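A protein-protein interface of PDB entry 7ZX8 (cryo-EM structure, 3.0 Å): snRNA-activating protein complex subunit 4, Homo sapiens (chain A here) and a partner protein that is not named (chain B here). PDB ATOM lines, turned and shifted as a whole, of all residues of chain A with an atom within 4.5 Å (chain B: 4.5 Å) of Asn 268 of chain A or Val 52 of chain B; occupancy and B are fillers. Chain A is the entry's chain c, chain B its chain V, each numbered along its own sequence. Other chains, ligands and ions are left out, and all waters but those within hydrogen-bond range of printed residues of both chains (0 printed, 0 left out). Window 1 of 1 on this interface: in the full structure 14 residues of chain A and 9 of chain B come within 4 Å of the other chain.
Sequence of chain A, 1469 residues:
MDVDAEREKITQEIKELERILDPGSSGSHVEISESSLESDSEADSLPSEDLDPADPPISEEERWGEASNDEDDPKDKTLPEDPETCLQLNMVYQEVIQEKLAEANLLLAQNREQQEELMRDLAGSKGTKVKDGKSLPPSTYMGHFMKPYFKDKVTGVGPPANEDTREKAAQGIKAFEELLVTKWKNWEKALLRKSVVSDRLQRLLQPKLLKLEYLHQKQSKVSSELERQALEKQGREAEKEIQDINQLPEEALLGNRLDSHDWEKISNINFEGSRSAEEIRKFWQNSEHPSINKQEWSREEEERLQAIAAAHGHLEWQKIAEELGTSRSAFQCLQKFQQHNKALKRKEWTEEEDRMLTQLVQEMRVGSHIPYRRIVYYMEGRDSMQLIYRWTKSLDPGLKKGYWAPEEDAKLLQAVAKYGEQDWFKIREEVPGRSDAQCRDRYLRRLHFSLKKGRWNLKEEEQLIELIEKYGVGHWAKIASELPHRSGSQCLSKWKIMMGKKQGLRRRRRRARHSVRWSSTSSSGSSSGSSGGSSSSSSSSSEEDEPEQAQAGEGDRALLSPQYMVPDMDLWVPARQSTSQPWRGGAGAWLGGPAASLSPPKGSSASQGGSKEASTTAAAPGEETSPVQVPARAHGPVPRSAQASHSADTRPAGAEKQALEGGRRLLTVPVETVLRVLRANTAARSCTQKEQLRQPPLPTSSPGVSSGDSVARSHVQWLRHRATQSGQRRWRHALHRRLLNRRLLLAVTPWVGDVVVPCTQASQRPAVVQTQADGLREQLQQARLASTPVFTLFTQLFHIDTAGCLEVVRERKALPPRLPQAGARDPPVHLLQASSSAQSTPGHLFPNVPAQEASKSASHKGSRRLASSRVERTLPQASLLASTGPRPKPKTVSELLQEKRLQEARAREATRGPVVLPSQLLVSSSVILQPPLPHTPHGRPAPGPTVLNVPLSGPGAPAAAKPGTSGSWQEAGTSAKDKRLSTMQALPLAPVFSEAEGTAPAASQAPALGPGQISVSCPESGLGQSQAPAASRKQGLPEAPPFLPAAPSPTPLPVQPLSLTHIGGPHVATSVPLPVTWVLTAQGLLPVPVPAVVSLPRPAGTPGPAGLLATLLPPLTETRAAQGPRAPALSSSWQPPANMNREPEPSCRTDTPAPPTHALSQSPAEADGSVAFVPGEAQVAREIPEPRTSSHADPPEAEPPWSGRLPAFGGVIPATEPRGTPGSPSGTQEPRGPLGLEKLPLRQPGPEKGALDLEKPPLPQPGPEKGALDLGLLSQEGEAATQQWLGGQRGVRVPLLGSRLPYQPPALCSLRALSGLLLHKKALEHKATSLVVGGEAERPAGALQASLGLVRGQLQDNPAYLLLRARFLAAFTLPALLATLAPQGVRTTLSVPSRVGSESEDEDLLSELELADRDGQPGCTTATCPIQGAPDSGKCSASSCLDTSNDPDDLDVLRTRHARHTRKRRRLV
The backbone carbonyl oxygen (O) of Gln 50 of chain B sits at hydrogen-bond distance from the side-chain amide nitrogen (ND2) of Asn 268 of chain A, at 3.1 Å. The guanidinium group (NH1) of Arg 51 of chain B is in salt-bridge range of the side-chain carboxylate (OE2) of Glu 264 of chain A (3.7 Å). The backbone carbonyl oxygen of Asn 268 of chain A lies within hydrogen-bond range of the guanidinium group of Arg 53 of chain B (3.2 Å). The backbone carbonyl oxygen of Glu 264 of chain A sits close to the backbone carbonyl oxygen of Gln 50 of chain B, 3.1 Å away.
O of Glu 264 of chain A sits at hydrogen-bond distance from ND2 of Asn 268 of chain A (2.7 Å). OD1 of Asn 268 of chain A is in hydrogen-bond range of OG of Ser 267 of chain A.
Among the printed residues, merely in contact across the chains: Lys 265 of chain A with Gln 50 of chain B, Asn 268 of chain A with Val 52 of chain B and Ile 269 of chain A with Gln 50 of chain B.
Asn 268 of chain A touches just these residues of chain B: Gln 50 (3.1 Å), Val 52 (3.8 Å) and Arg 53 (3.2 Å). Val 52 of chain B touches just one residue of chain A: Asn 268 (3.8 Å). Printed residues of chain B within 4 Å of Lys 265 of chain A: Gln 50 (3.4 Å). Printed residues of chain A within 4 Å of Arg 51 of chain B: Glu 264. Ala 49 of chain B touches none of the printed residues of chain A. The nearest residue of chain B that does not touch Asn 268 of chain A is Arg 51 of chain B (4.1 Å). The nearest printed residue of chain B that does not touch Glu 264 of chain A is Val 52 of chain B (5.4 Å).
Of the 6 printed residues of chain B, 4 touch a printed residue of chain A. Printed residues of chain B that touch a printed residue of chain A: Gln 50, Arg 51, Val 52 and Arg 53. Of the 8 printed residues of chain A, 4 touch a printed residue of chain B. Printed residues of chain A that touch a printed residue of chain B: Glu 264, Lys 265, Asn 268 and Ile 269. Hydrophobic or aromatic side chains of chain A that line the printed part of chain B: Ile 269. Among the printed residues, 7 pairs touch across the chains. Among the printed residues, Asp or Glu carboxylates within 4 Å of a Lys or Arg side-chain nitrogen of the other chain: Glu 264 of chain A with Arg 51 of chain B.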
ATOM      1  N   GLU A 264      11.583   7.608  -8.303  1.00  0.00           N
ATOM      2  CA  GLU A 264      12.492   7.278  -9.388  1.00  0.00           C
ATOM      3  C   GLU A 264      11.900   7.652 -10.739  1.00  0.00           C
ATOM      4  O   GLU A 264      12.647   7.843 -11.704  1.00  0.00           O
ATOM      5  CB  GLU A 264      12.831   5.796  -9.330  1.00  0.00           C
ATOM      6  CG  GLU A 264      11.626   4.908  -9.490  1.00  0.00           C
ATOM      7  CD  GLU A 264      11.937   3.460  -9.205  1.00  0.00           C
ATOM      8  OE1 GLU A 264      13.097   3.162  -8.854  1.00  0.00           O
ATOM      9  OE2 GLU A 264      11.019   2.622  -9.323  1.00  0.00           O
ATOM     10  N   LYS A 265      10.575   7.765 -10.825  1.00  0.00           N
ATOM     11  CA  LYS A 265       9.958   8.319 -12.025  1.00  0.00           C
ATOM     12  C   LYS A 265      10.129   9.829 -12.061  1.00  0.00           C
ATOM     13  O   LYS A 265      10.372  10.414 -13.122  1.00  0.00           O
ATOM     14  CB  LYS A 265       8.477   7.943 -12.075  1.00  0.00           C
ATOM     15  CG  LYS A 265       7.750   8.407 -13.320  1.00  0.00           C
ATOM     16  CD  LYS A 265       6.308   7.950 -13.305  1.00  0.00           C
ATOM     17  CE  LYS A 265       5.548   8.421 -14.530  1.00  0.00           C
ATOM     18  NZ  LYS A 265       4.129   7.967 -14.510  1.00  0.00           N
ATOM     19  N   ILE A 266      10.007  10.476 -10.902  1.00  0.00           N
ATOM     20  CA  ILE A 266      10.215  11.917 -10.832  1.00  0.00           C
ATOM     21  C   ILE A 266      11.614  12.277 -11.293  1.00  0.00           C
ATOM     22  O   ILE A 266      11.794  13.074 -12.220  1.00  0.00           O
ATOM     23  CB  ILE A 266       9.957  12.426  -9.405  1.00  0.00           C
ATOM     24  CG1 ILE A 266       8.474  12.351  -9.072  1.00  0.00           C
ATOM     25  CG2 ILE A 266      10.455  13.835  -9.256  1.00  0.00           C
ATOM     26  CD1 ILE A 266       8.143  12.867  -7.704  1.00  0.00           C
ATOM     27  N   SER A 267      12.625  11.689 -10.658  1.00  0.00           N
ATOM     28  CA  SER A 267      14.008  12.066 -10.905  1.00  0.00           C
ATOM     29  C   SER A 267      14.421  11.879 -12.355  1.00  0.00           C
ATOM     30  O   SER A 267      15.393  12.502 -12.793  1.00  0.00           O
ATOM     31  CB  SER A 267      14.939  11.256 -10.014  1.00  0.00           C
ATOM     32  OG  SER A 267      15.296  10.046 -10.651  1.00  0.00           O
ATOM     33  N   ASN A 268      13.721  11.038 -13.107  1.00  0.00           N
ATOM     34  CA  ASN A 268      14.063  10.807 -14.502  1.00  0.00           C
ATOM     35  C   ASN A 268      13.131  11.496 -15.480  1.00  0.00           C
ATOM     36  O   ASN A 268      13.489  11.646 -16.648  1.00  0.00           O
ATOM     37  CB  ASN A 268      14.075   9.308 -14.799  1.00  0.00           C
ATOM     38  CG  ASN A 268      14.834   8.530 -13.762  1.00  0.00           C
ATOM     39  OD1 ASN A 268      15.727   9.065 -13.108  1.00  0.00           O
ATOM     40  ND2 ASN A 268      14.479   7.266 -13.587  1.00  0.00           N
ATOM     41  N   ILE A 269      11.952  11.918 -15.040  1.00  0.00           N
ATOM     42  CA  ILE A 269      11.005  12.588 -15.913  1.00  0.00           C
ATOM     43  C   ILE A 269      10.911  14.075 -15.606  1.00  0.00           C
ATOM     44  O   ILE A 269      11.269  14.903 -16.441  1.00  0.00           O
ATOM     45  CB  ILE A 269       9.624  11.907 -15.814  1.00  0.00           C
ATOM     46  CG1 ILE A 269       9.728  10.457 -16.282  1.00  0.00           C
ATOM     47  CG2 ILE A 269       8.599  12.660 -16.635  1.00  0.00           C
ATOM     48  CD1 ILE A 269      10.431  10.302 -17.609  1.00  0.00           C
ATOM     49  N   ASN A 270      10.452  14.436 -14.412  1.00  0.00           N
ATOM     50  CA  ASN A 270      10.384  15.843 -14.052  1.00  0.00           C
ATOM     51  C   ASN A 270      11.752  16.473 -13.888  1.00  0.00           C
ATOM     52  O   ASN A 270      12.004  17.537 -14.459  1.00  0.00           O
ATOM     53  CB  ASN A 270       9.587  16.025 -12.761  1.00  0.00           C
ATOM     54  CG  ASN A 270       8.102  15.971 -12.994  1.00  0.00           C
ATOM     55  OD1 ASN A 270       7.540  14.904 -13.231  1.00  0.00           O
ATOM     56  ND2 ASN A 270       7.449  17.122 -12.917  1.00  0.00           N
ATOM     57  N   PHE A 271      12.638  15.844 -13.134  1.00  0.00           N
ATOM     58  CA  PHE A 271      14.018  16.286 -13.075  1.00  0.00           C
ATOM     59  C   PHE A 271      14.812  15.599 -14.171  1.00  0.00           C
ATOM     60  O   PHE A 271      14.507  14.480 -14.591  1.00  0.00           O
ATOM     61  CB  PHE A 271      14.633  15.993 -11.710  1.00  0.00           C
ATOM     62  CG  PHE A 271      14.034  16.791 -10.600  1.00  0.00           C
ATOM     63  CD1 PHE A 271      12.788  16.480 -10.102  1.00  0.00           C
ATOM     64  CD2 PHE A 271      14.715  17.855 -10.058  1.00  0.00           C
ATOM     65  CE1 PHE A 271      12.232  17.212  -9.082  1.00  0.00           C
ATOM     66  CE2 PHE A 271      14.163  18.590  -9.037  1.00  0.00           C
ATOM     67  CZ  PHE A 271      12.919  18.268  -8.548  1.00  0.00           C
ATOM     68  N   ALA B  49      10.622   2.051 -18.721  1.00  0.00           N
ATOM     69  CA  ALA B  49      11.142   3.284 -19.353  1.00  0.00           C
ATOM     70  C   ALA B  49      11.746   4.245 -18.323  1.00  0.00           C
ATOM     71  O   ALA B  49      12.970   4.472 -18.388  1.00  0.00           O
ATOM     72  CB  ALA B  49      10.023   3.968 -20.103  1.00  0.00           C
ATOM     73  N   GLN B  50      10.930   4.774 -17.407  1.00  0.00           N
ATOM     74  CA  GLN B  50      11.422   5.836 -16.488  1.00  0.00           C
ATOM     75  C   GLN B  50      11.601   5.343 -15.050  1.00  0.00           C
ATOM     76  O   GLN B  50      11.588   6.201 -14.147  1.00  0.00           O
ATOM     77  CB  GLN B  50      10.407   6.977 -16.502  1.00  0.00           C
ATOM     78  CG  GLN B  50       9.498   6.944 -17.722  1.00  0.00           C
ATOM     79  CD  GLN B  50       8.048   6.755 -17.352  1.00  0.00           C
ATOM     80  OE1 GLN B  50       7.720   6.400 -16.224  1.00  0.00           O
ATOM     81  NE2 GLN B  50       7.165   6.989 -18.309  1.00  0.00           N
ATOM     82  N   ARG B  51      11.775   4.039 -14.832  1.00  0.00           N
ATOM     83  CA  ARG B  51      12.056   3.575 -13.444  1.00  0.00           C
ATOM     84  C   ARG B  51      13.554   3.309 -13.261  1.00  0.00           C
ATOM     85  O   ARG B  51      13.954   3.027 -12.114  1.00  0.00           O
ATOM     86  CB  ARG B  51      11.241   2.325 -13.099  1.00  0.00           C
ATOM     87  CG  ARG B  51       9.735   2.542 -13.035  1.00  0.00           C
ATOM     88  CD  ARG B  51       8.918   1.330 -12.625  1.00  0.00           C
ATOM     89  NE  ARG B  51       7.484   1.586 -12.603  1.00  0.00           N
ATOM     90  CZ  ARG B  51       6.832   2.148 -11.591  1.00  0.00           C
ATOM     91  NH1 ARG B  51       7.485   2.511 -10.502  1.00  0.00           N
ATOM     92  NH2 ARG B  51       5.528   2.337 -11.667  1.00  0.00           N
ATOM     93  N   VAL B  52      14.352   3.399 -14.332  1.00  0.00           N
ATOM     94  CA  VAL B  52      15.800   3.037 -14.228  1.00  0.00           C
ATOM     95  C   VAL B  52      16.663   4.028 -15.016  1.00  0.00           C
ATOM     96  O   VAL B  52      16.108   4.710 -15.901  1.00  0.00           O
ATOM     97  CB  VAL B  52      16.048   1.594 -14.703  1.00  0.00           C
ATOM     98  CG1 VAL B  52      17.531   1.260 -14.716  1.00  0.00           C
ATOM     99  CG2 VAL B  52      15.273   0.587 -13.868  1.00  0.00           C
ATOM    100  N   ARG B  53      17.961   4.104 -14.693  1.00  0.00           N
ATOM    101  CA  ARG B  53      18.906   4.987 -15.435  1.00  0.00           C
ATOM    102  C   ARG B  53      20.343   4.515 -15.178  1.00  0.00           C
ATOM    103  O   ARG B  53      21.106   5.281 -14.556  1.00  0.00           O
ATOM    104  CB  ARG B  53      18.727   6.450 -15.015  1.00  0.00           C
ATOM    105  CG  ARG B  53      19.572   7.431 -15.813  1.00  0.00           C
ATOM    106  CD  ARG B  53      19.404   8.861 -15.337  1.00  0.00           C
ATOM    107  NE  ARG B  53      18.053   9.355 -15.554  1.00  0.00           N
ATOM    108  CZ  ARG B  53      17.615   9.873 -16.696  1.00  0.00           C
ATOM    109  NH1 ARG B  53      18.426   9.963 -17.737  1.00  0.00           N
ATOM    110  NH2 ARG B  53      16.368  10.296 -16.795  1.00  0.00           N
ATOM    111  N   ASN B  54      20.698   3.307 -15.636  1.00  0.00           N
ATOM    112  CA  ASN B  54      22.039   2.767 -15.430  1.00  0.00           C
ATOM    113  C   ASN B  54      22.619   2.478 -16.809  1.00  0.00           C
ATOM    114  O   ASN B  54      22.005   1.775 -17.617  1.00  0.00           O
ATOM    115  CB  ASN B  54      22.030   1.538 -14.506  1.00  0.00           C
ATOM    116  CG  ASN B  54      21.724   0.226 -15.221  1.00  0.00           C
ATOM    117  OD1 ASN B  54      21.104   0.198 -16.280  1.00  0.00           O
ATOM    118  ND2 ASN B  54      22.176  -0.874 -14.633  1.00  0.00           N
